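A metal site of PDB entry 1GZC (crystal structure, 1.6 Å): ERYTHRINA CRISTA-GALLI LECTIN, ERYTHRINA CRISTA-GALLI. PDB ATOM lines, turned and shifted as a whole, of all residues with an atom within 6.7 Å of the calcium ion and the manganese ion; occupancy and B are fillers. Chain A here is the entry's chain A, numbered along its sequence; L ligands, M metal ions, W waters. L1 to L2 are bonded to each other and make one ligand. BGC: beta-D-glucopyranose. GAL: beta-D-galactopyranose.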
ATOM      1  N   ASP A  89     -12.937 -20.991  -1.573  1.00  0.00           N
ATOM      2  CA  ASP A  89     -13.493 -20.717  -0.243  1.00  0.00           C
ATOM      3  C   ASP A  89     -12.608 -21.338   0.853  1.00  0.00           C
ATOM      4  O   ASP A  89     -12.647 -20.873   1.974  1.00  0.00           O
ATOM      5  CB  ASP A  89     -14.888 -21.311  -0.131  1.00  0.00           C
ATOM      6  CG  ASP A  89     -15.999 -20.298  -0.492  1.00  0.00           C
ATOM      7  OD1 ASP A  89     -16.218 -19.367   0.343  1.00  0.00           O
ATOM      8  OD2 ASP A  89     -16.630 -20.433  -1.595  1.00  0.00           O
ATOM      9  N   TYR A 106     -19.352 -23.818  -1.332  1.00  0.00           N
ATOM     10  CA  TYR A 106     -18.964 -22.422  -1.068  1.00  0.00           C
ATOM     11  C   TYR A 106     -18.427 -22.288   0.362  1.00  0.00           C
ATOM     12  O   TYR A 106     -17.565 -23.081   0.764  1.00  0.00           O
ATOM     13  CB  TYR A 106     -20.144 -21.455  -1.334  1.00  0.00           C
ATOM     14  CG  TYR A 106     -20.745 -21.633  -2.721  1.00  0.00           C
ATOM     15  CD1 TYR A 106     -19.944 -21.896  -3.819  1.00  0.00           C
ATOM     16  CD2 TYR A 106     -22.138 -21.541  -2.925  1.00  0.00           C
ATOM     17  CE1 TYR A 106     -20.505 -22.065  -5.112  1.00  0.00           C
ATOM     18  CE2 TYR A 106     -22.708 -21.716  -4.187  1.00  0.00           C
ATOM     19  CZ  TYR A 106     -21.885 -21.978  -5.265  1.00  0.00           C
ATOM     20  OH  TYR A 106     -22.466 -22.179  -6.504  1.00  0.00           O
ATOM     21  N   GLY A 107     -18.917 -21.303   1.131  1.00  0.00           N
ATOM     22  CA  GLY A 107     -18.399 -21.110   2.473  1.00  0.00           C
ATOM     23  C   GLY A 107     -18.669 -22.222   3.470  1.00  0.00           C
ATOM     24  O   GLY A 107     -18.104 -22.205   4.584  1.00  0.00           O
ATOM     25  N   TYR A 108     -19.530 -23.186   3.110  1.00  0.00           N
ATOM     26  CA  TYR A 108     -19.811 -24.319   3.998  1.00  0.00           C
ATOM     27  C   TYR A 108     -18.795 -25.448   3.810  1.00  0.00           C
ATOM     28  O   TYR A 108     -18.838 -26.453   4.546  1.00  0.00           O
ATOM     29  CB  TYR A 108     -21.249 -24.808   3.798  1.00  0.00           C
ATOM     30  CG  TYR A 108     -22.230 -23.675   4.027  1.00  0.00           C
ATOM     31  CD1 TYR A 108     -22.309 -23.053   5.247  1.00  0.00           C
ATOM     32  CD2 TYR A 108     -23.053 -23.223   3.006  1.00  0.00           C
ATOM     33  CE1 TYR A 108     -23.196 -21.968   5.480  1.00  0.00           C
ATOM     34  CE2 TYR A 108     -23.950 -22.134   3.229  1.00  0.00           C
ATOM     35  CZ  TYR A 108     -23.990 -21.532   4.463  1.00  0.00           C
ATOM     36  OH  TYR A 108     -24.813 -20.430   4.707  1.00  0.00           O
ATOM     37  N   LEU A 109     -17.896 -25.245   2.829  1.00  0.00           N
ATOM     38  CA  LEU A 109     -16.701 -26.080   2.571  1.00  0.00           C
ATOM     39  C   LEU A 109     -16.959 -27.570   2.336  1.00  0.00           C
ATOM     40  O   LEU A 109     -16.078 -28.393   2.532  1.00  0.00           O
ATOM     41  CB  LEU A 109     -15.721 -25.967   3.766  1.00  0.00           C
ATOM     42  CG  LEU A 109     -15.360 -24.498   4.052  1.00  0.00           C
ATOM     43  CD1 LEU A 109     -14.454 -24.439   5.298  1.00  0.00           C
ATOM     44  CD2 LEU A 109     -14.637 -23.833   2.836  1.00  0.00           C
ATOM     45  N   GLU A 127     -10.638 -25.916   9.871  1.00  0.00           N
ATOM     46  CA  GLU A 127     -10.659 -25.283   8.543  1.00  0.00           C
ATOM     47  C   GLU A 127      -9.501 -24.339   8.260  1.00  0.00           C
ATOM     48  O   GLU A 127      -8.904 -23.783   9.192  1.00  0.00           O
ATOM     49  CB  GLU A 127     -11.963 -24.497   8.438  1.00  0.00           C
ATOM     50  CG  GLU A 127     -12.051 -23.355   9.494  1.00  0.00           C
ATOM     51  CD  GLU A 127     -13.222 -22.389   9.227  1.00  0.00           C
ATOM     52  OE1 GLU A 127     -14.352 -22.876   9.056  1.00  0.00           O
ATOM     53  OE2 GLU A 127     -12.978 -21.138   9.228  1.00  0.00           O
ATOM     54  N   ASP A 129      -9.590 -21.360   5.936  1.00  0.00           N
ATOM     55  CA  ASP A 129     -10.642 -20.594   5.253  1.00  0.00           C
ATOM     56  C   ASP A 129     -10.114 -19.350   4.573  1.00  0.00           C
ATOM     57  O   ASP A 129      -9.479 -18.499   5.213  1.00  0.00           O
ATOM     58  CB  ASP A 129     -11.638 -20.204   6.354  1.00  0.00           C
ATOM     59  CG  ASP A 129     -12.936 -19.559   5.845  1.00  0.00           C
ATOM     60  OD1 ASP A 129     -13.027 -19.224   4.685  1.00  0.00           O
ATOM     61  OD2 ASP A 129     -13.891 -19.424   6.664  1.00  0.00           O
ATOM     62  N   THR A 130     -10.401 -19.237   3.275  1.00  0.00           N
ATOM     63  CA  THR A 130      -9.864 -18.154   2.487  1.00  0.00           C
ATOM     64  C   THR A 130     -10.819 -17.033   2.098  1.00  0.00           C
ATOM     65  O   THR A 130     -10.365 -16.054   1.471  1.00  0.00           O
ATOM     66  CB  THR A 130      -9.268 -18.746   1.221  1.00  0.00           C
ATOM     67  OG1 THR A 130     -10.305 -19.494   0.566  1.00  0.00           O
ATOM     68  CG2 THR A 130      -8.103 -19.738   1.586  1.00  0.00           C
ATOM     69  N   PHE A 131     -12.088 -17.124   2.482  1.00  0.00           N
ATOM     70  CA  PHE A 131     -13.054 -16.094   2.120  1.00  0.00           C
ATOM     71  C   PHE A 131     -13.833 -15.692   3.350  1.00  0.00           C
ATOM     72  O   PHE A 131     -14.355 -16.555   4.055  1.00  0.00           O
ATOM     73  CB  PHE A 131     -14.016 -16.626   1.023  1.00  0.00           C
ATOM     74  CG  PHE A 131     -15.019 -15.586   0.572  1.00  0.00           C
ATOM     75  CD1 PHE A 131     -14.705 -14.697  -0.480  1.00  0.00           C
ATOM     76  CD2 PHE A 131     -16.219 -15.456   1.255  1.00  0.00           C
ATOM     77  CE1 PHE A 131     -15.620 -13.666  -0.834  1.00  0.00           C
ATOM     78  CE2 PHE A 131     -17.146 -14.451   0.925  1.00  0.00           C
ATOM     79  CZ  PHE A 131     -16.830 -13.552  -0.124  1.00  0.00           C
ATOM     80  N   SER A 132     -13.913 -14.374   3.613  1.00  0.00           N
ATOM     81  CA  SER A 132     -14.637 -13.915   4.795  1.00  0.00           C
ATOM     82  C   SER A 132     -16.161 -13.790   4.554  1.00  0.00           C
ATOM     83  O   SER A 132     -16.645 -12.799   3.962  1.00  0.00           O
ATOM     84  CB  SER A 132     -14.083 -12.556   5.280  1.00  0.00           C
ATOM     85  OG  SER A 132     -14.661 -12.251   6.547  1.00  0.00           O
ATOM     86  N   ASN A 133     -16.913 -14.807   4.965  1.00  0.00           N
ATOM     87  CA  ASN A 133     -18.358 -14.851   4.870  1.00  0.00           C
ATOM     88  C   ASN A 133     -18.987 -14.001   6.023  1.00  0.00           C
ATOM     89  O   ASN A 133     -18.279 -13.498   6.925  1.00  0.00           O
ATOM     90  CB  ASN A 133     -18.835 -16.316   4.986  1.00  0.00           C
ATOM     91  CG  ASN A 133     -18.385 -17.147   3.836  1.00  0.00           C
ATOM     92  OD1 ASN A 133     -17.333 -17.820   3.879  1.00  0.00           O
ATOM     93  ND2 ASN A 133     -19.160 -17.095   2.751  1.00  0.00           N
ATOM     94  N   TRP A 135     -20.499 -14.846   8.639  1.00  0.00           N
ATOM     95  CA  TRP A 135     -20.226 -15.413   9.954  1.00  0.00           C
ATOM     96  C   TRP A 135     -18.737 -15.503  10.320  1.00  0.00           C
ATOM     97  O   TRP A 135     -18.403 -15.988  11.375  1.00  0.00           O
ATOM     98  CB  TRP A 135     -20.795 -16.845  10.010  1.00  0.00           C
ATOM     99  CG  TRP A 135     -20.218 -17.728   8.891  1.00  0.00           C
ATOM    100  CD1 TRP A 135     -18.984 -18.375   8.882  1.00  0.00           C
ATOM    101  CD2 TRP A 135     -20.823 -17.998   7.614  1.00  0.00           C
ATOM    102  NE1 TRP A 135     -18.807 -19.015   7.663  1.00  0.00           N
ATOM    103  CE2 TRP A 135     -19.909 -18.810   6.875  1.00  0.00           C
ATOM    104  CE3 TRP A 135     -22.038 -17.639   7.020  1.00  0.00           C
ATOM    105  CZ2 TRP A 135     -20.196 -19.257   5.585  1.00  0.00           C
ATOM    106  CZ3 TRP A 135     -22.314 -18.078   5.732  1.00  0.00           C
ATOM    107  CH2 TRP A 135     -21.387 -18.890   5.024  1.00  0.00           C
ATOM    108  N   ASP A 136     -17.869 -15.024   9.460  1.00  0.00           N
ATOM    109  CA  ASP A 136     -16.409 -15.148   9.663  1.00  0.00           C
ATOM    110  C   ASP A 136     -15.734 -13.901  10.215  1.00  0.00           C
ATOM    111  O   ASP A 136     -16.282 -12.806  10.123  1.00  0.00           O
ATOM    112  CB  ASP A 136     -15.722 -15.337   8.289  1.00  0.00           C
ATOM    113  CG  ASP A 136     -15.731 -16.774   7.788  1.00  0.00           C
ATOM    114  OD1 ASP A 136     -15.527 -17.668   8.618  1.00  0.00           O
ATOM    115  OD2 ASP A 136     -15.907 -16.986   6.570  1.00  0.00           O
ATOM    116  N   PRO A 137     -14.514 -14.074  10.778  1.00  0.00           N
ATOM    117  CA  PRO A 137     -13.757 -12.916  11.260  1.00  0.00           C
ATOM    118  C   PRO A 137     -13.300 -12.326   9.909  1.00  0.00           C
ATOM    119  O   PRO A 137     -13.344 -13.001   8.877  1.00  0.00           O
ATOM    120  CB  PRO A 137     -12.588 -13.560  12.035  1.00  0.00           C
ATOM    121  CG  PRO A 137     -12.447 -14.968  11.339  1.00  0.00           C
ATOM    122  CD  PRO A 137     -13.905 -15.353  11.190  1.00  0.00           C
ATOM    123  N   VAL A 140      -8.530 -13.039   6.407  1.00  0.00           N
ATOM    124  CA  VAL A 140      -8.412 -14.276   5.635  1.00  0.00           C
ATOM    125  C   VAL A 140      -7.019 -14.288   4.977  1.00  0.00           C
ATOM    126  O   VAL A 140      -6.472 -13.273   4.543  1.00  0.00           O
ATOM    127  CB  VAL A 140      -9.492 -14.449   4.562  1.00  0.00           C
ATOM    128  CG1 VAL A 140     -10.817 -14.878   5.216  1.00  0.00           C
ATOM    129  CG2 VAL A 140      -9.705 -13.139   3.756  1.00  0.00           C
ATOM    130  N   HIS A 142      -7.675 -17.763   7.495  1.00  0.00           N
ATOM    131  CA  HIS A 142      -7.625 -18.037   8.913  1.00  0.00           C
ATOM    132  C   HIS A 142      -7.789 -19.534   9.183  1.00  0.00           C
ATOM    133  O   HIS A 142      -8.453 -20.246   8.438  1.00  0.00           O
ATOM    134  CB  HIS A 142      -8.709 -17.262   9.743  1.00  0.00           C
ATOM    135  CG  HIS A 142     -10.143 -17.438   9.278  1.00  0.00           C
ATOM    136  ND1 HIS A 142     -10.785 -16.549   8.434  1.00  0.00           N
ATOM    137  CD2 HIS A 142     -11.048 -18.397   9.576  1.00  0.00           C
ATOM    138  CE1 HIS A 142     -12.030 -16.965   8.226  1.00  0.00           C
ATOM    139  NE2 HIS A 142     -12.217 -18.087   8.904  1.00  0.00           N
ATOM    140  N   ILE A 143      -7.174 -19.992  10.274  1.00  0.00           N
ATOM    141  CA  ILE A 143      -7.405 -21.366  10.748  1.00  0.00           C
ATOM    142  C   ILE A 143      -8.629 -21.234  11.630  1.00  0.00           C
ATOM    143  O   ILE A 143      -8.774 -20.223  12.360  1.00  0.00           O
ATOM    144  CB  ILE A 143      -6.226 -21.861  11.627  1.00  0.00           C
ATOM    145  CG1 ILE A 143      -4.913 -21.718  10.840  1.00  0.00           C
ATOM    146  CG2 ILE A 143      -6.394 -23.336  11.934  1.00  0.00           C
ATOM    147  CD1 ILE A 143      -3.712 -22.169  11.658  1.00  0.00           C
ATOM    148  N   GLY A 144      -9.508 -22.231  11.594  1.00  0.00           N
ATOM    149  CA  GLY A 144     -10.687 -22.209  12.464  1.00  0.00           C
ATOM    150  C   GLY A 144     -10.985 -23.572  13.090  1.00  0.00           C
ATOM    151  O   GLY A 144     -10.797 -24.625  12.450  1.00  0.00           O
ATOM    152  N   ASP A 146     -13.977 -25.680  14.299  1.00  0.00           N
ATOM    153  CA  ASP A 146     -15.436 -25.737  14.066  1.00  0.00           C
ATOM    154  C   ASP A 146     -16.050 -26.908  14.802  1.00  0.00           C
ATOM    155  O   ASP A 146     -15.738 -28.083  14.528  1.00  0.00           O
ATOM    156  CB  ASP A 146     -15.703 -25.929  12.567  1.00  0.00           C
ATOM    157  CG  ASP A 146     -15.128 -24.808  11.694  1.00  0.00           C
ATOM    158  OD1 ASP A 146     -14.649 -23.790  12.243  1.00  0.00           O
ATOM    159  OD2 ASP A 146     -15.184 -24.946  10.440  1.00  0.00           O
ATOM    160  N   ILE A 150     -20.195 -24.038  11.138  1.00  0.00           N
ATOM    161  CA  ILE A 150     -19.209 -23.378  10.272  1.00  0.00           C
ATOM    162  C   ILE A 150     -18.753 -22.053  10.981  1.00  0.00           C
ATOM    163  O   ILE A 150     -17.758 -21.455  10.566  1.00  0.00           O
ATOM    164  CB  ILE A 150     -19.830 -23.067   8.879  1.00  0.00           C
ATOM    165  CG1 ILE A 150     -18.764 -22.616   7.888  1.00  0.00           C
ATOM    166  CG2 ILE A 150     -20.830 -21.863   9.015  1.00  0.00           C
ATOM    167  CD1 ILE A 150     -17.694 -23.721   7.580  1.00  0.00           C
ATOM    168  N   ARG A 151     -19.461 -21.611  12.022  1.00  0.00           N
ATOM    169  CA  ARG A 151     -19.048 -20.375  12.739  1.00  0.00           C
ATOM    170  C   ARG A 151     -18.082 -20.863  13.838  1.00  0.00           C
ATOM    171  O   ARG A 151     -18.486 -21.345  14.916  1.00  0.00           O
ATOM    172  CB  ARG A 151     -20.272 -19.697  13.392  1.00  0.00           C
ATOM    173  CG  ARG A 151     -21.361 -19.416  12.396  1.00  0.00           C
ATOM    174  CD  ARG A 151     -22.379 -18.398  12.989  1.00  0.00           C
ATOM    175  NE  ARG A 151     -23.447 -18.132  12.030  1.00  0.00           N
ATOM    176  CZ  ARG A 151     -23.933 -16.924  11.759  1.00  0.00           C
ATOM    177  NH1 ARG A 151     -23.440 -15.870  12.400  1.00  0.00           N
ATOM    178  NH2 ARG A 151     -24.816 -16.777  10.779  1.00  0.00           N
ATOM    179  N   SER A 152     -16.799 -20.725  13.540  1.00  0.00           N
ATOM    180  CA  SER A 152     -15.766 -21.262  14.434  1.00  0.00           C
ATOM    181  C   SER A 152     -15.834 -20.749  15.852  1.00  0.00           C
ATOM    182  O   SER A 152     -16.099 -19.567  16.074  1.00  0.00           O
ATOM    183  CB  SER A 152     -14.359 -20.907  13.921  1.00  0.00           C
ATOM    184  OG  SER A 152     -14.195 -21.193  12.533  1.00  0.00           O
ATOM    185  N   THR A 155     -10.581 -18.761  16.017  1.00  0.00           N
ATOM    186  CA  THR A 155      -9.830 -18.651  14.777  1.00  0.00           C
ATOM    187  C   THR A 155      -8.461 -18.020  15.000  1.00  0.00           C
ATOM    188  O   THR A 155      -8.206 -17.356  16.019  1.00  0.00           O
ATOM    189  CB  THR A 155     -10.567 -17.806  13.728  1.00  0.00           C
ATOM    190  OG1 THR A 155     -10.803 -16.458  14.245  1.00  0.00           O
ATOM    191  CG2 THR A 155     -11.894 -18.452  13.416  1.00  0.00           C
HETATM  192  C2  BGC L   1     -22.556 -13.486  -5.648  1.00  0.00           C
HETATM  193  C3  BGC L   1     -21.948 -14.765  -5.007  1.00  0.00           C
HETATM  194  C4  BGC L   1     -22.139 -14.743  -3.484  1.00  0.00           C
HETATM  195  C5  BGC L   1     -23.620 -14.558  -3.095  1.00  0.00           C
HETATM  196  C6  BGC L   1     -23.785 -14.348  -1.583  1.00  0.00           C
HETATM  197  C1  BGC L   1     -24.024 -13.423  -5.242  1.00  0.00           C
HETATM  198  O1  BGC L   1     -24.604 -12.279  -5.797  1.00  0.00           O
HETATM  199  O2  BGC L   1     -22.386 -13.579  -7.055  1.00  0.00           O
HETATM  200  O3  BGC L   1     -20.570 -14.845  -5.371  1.00  0.00           O
HETATM  201  O4  BGC L   1     -21.711 -16.012  -2.843  1.00  0.00           O
HETATM  202  O5  BGC L   1     -24.110 -13.340  -3.779  1.00  0.00           O
HETATM  203  O6  BGC L   1     -25.161 -14.253  -1.235  1.00  0.00           O
HETATM  204  C1  GAL L   2     -20.437 -16.014  -2.171  1.00  0.00           C
HETATM  205  C2  GAL L   2     -20.304 -17.271  -1.317  1.00  0.00           C
HETATM  206  C3  GAL L   2     -18.871 -17.225  -0.649  1.00  0.00           C
HETATM  207  C4  GAL L   2     -17.819 -17.147  -1.766  1.00  0.00           C
HETATM  208  C5  GAL L   2     -18.077 -15.908  -2.631  1.00  0.00           C
HETATM  209  C6  GAL L   2     -17.119 -15.808  -3.810  1.00  0.00           C
HETATM  210  O2  GAL L   2     -21.332 -17.332  -0.311  1.00  0.00           O
HETATM  211  O3  GAL L   2     -18.694 -18.375   0.172  1.00  0.00           O
HETATM  212  O4  GAL L   2     -17.874 -18.260  -2.651  1.00  0.00           O
HETATM  213  O5  GAL L   2     -19.418 -15.951  -3.176  1.00  0.00           O
HETATM  214  O6  GAL L   2     -17.247 -14.489  -4.356  1.00  0.00           O
HETATM  215 CA    CA M   1     -15.354 -18.539   4.888  1.00  0.00          CA
HETATM  216 MN    MN M   2     -14.142 -19.343   8.810  1.00  0.00          MN
HETATM  217  O   HOH W   1     -15.852 -20.770   8.554  1.00  0.00           O
HETATM  218  O   HOH W   2     -16.652 -20.347   5.838  1.00  0.00           O
HETATM  219  O   HOH W   3     -14.487 -19.067  10.953  1.00  0.00           O
HETATM  220  O   HOH W   4     -15.125 -19.623   2.771  1.00  0.00           O
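An oxygen (O3) of GAL L2 sits at hydrogen-bond distance from the side-chain amide nitrogen (ND2) of Asn 133, at 2.9 Å.
O3 of GAL L2 lies within hydrogen-bond range of N of Gly 107, at 3.1 Å.
O3 of GAL L2 is in hydrogen-bond range of OD1 of Asp 89 (2.7 Å).
The backbone carbonyl oxygen of Gly 144 is in hydrogen-bond range of the backbone NH of Glu 127 (2.9 Å).
The side-chain carboxylate (OD2) of Asp 146 lies close to the side-chain carboxylate (OE1) of Glu 127, 2.6 Å away.
Four residues have an atom within 4 Å of the manganese ion: Glu 127, Asp 129, Asp 136 and His 142.
The nearest printed residue that does not touch the manganese ion is Ser 152 (4.2 Å).
The calcium ion is bound by OD1 of Asn 133 (2.3 Å), OD2 of Asp 136 (2.4 Å), O of Phe 131 (2.4 Å), water W4 (2.4 Å), water W2 (2.4 Å), OD1 of Asp 129 (2.4 Å) and OD2 of Asp 129 (2.5 Å).
The calcium ion has seven donor atoms within binding distance.
The manganese ion is bound by OD2 of Asp 129 (2.2 Å), OE2 of Glu 127 (2.2 Å), OD1 of Asp 136 (2.2 Å), water W3 (2.2 Å), water W1 (2.2 Å) and NE2 of His 142 (2.3 Å).
The manganese ion has six donor atoms within binding distance.
Water W2 bridges O of Gly 107 and NE1 of Trp 135.
Water W1 bridges the side-chain carboxylate of Glu 127 (2.6 Å) and the backbone carbonyl oxygen of Ile 150 (2.9 Å).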
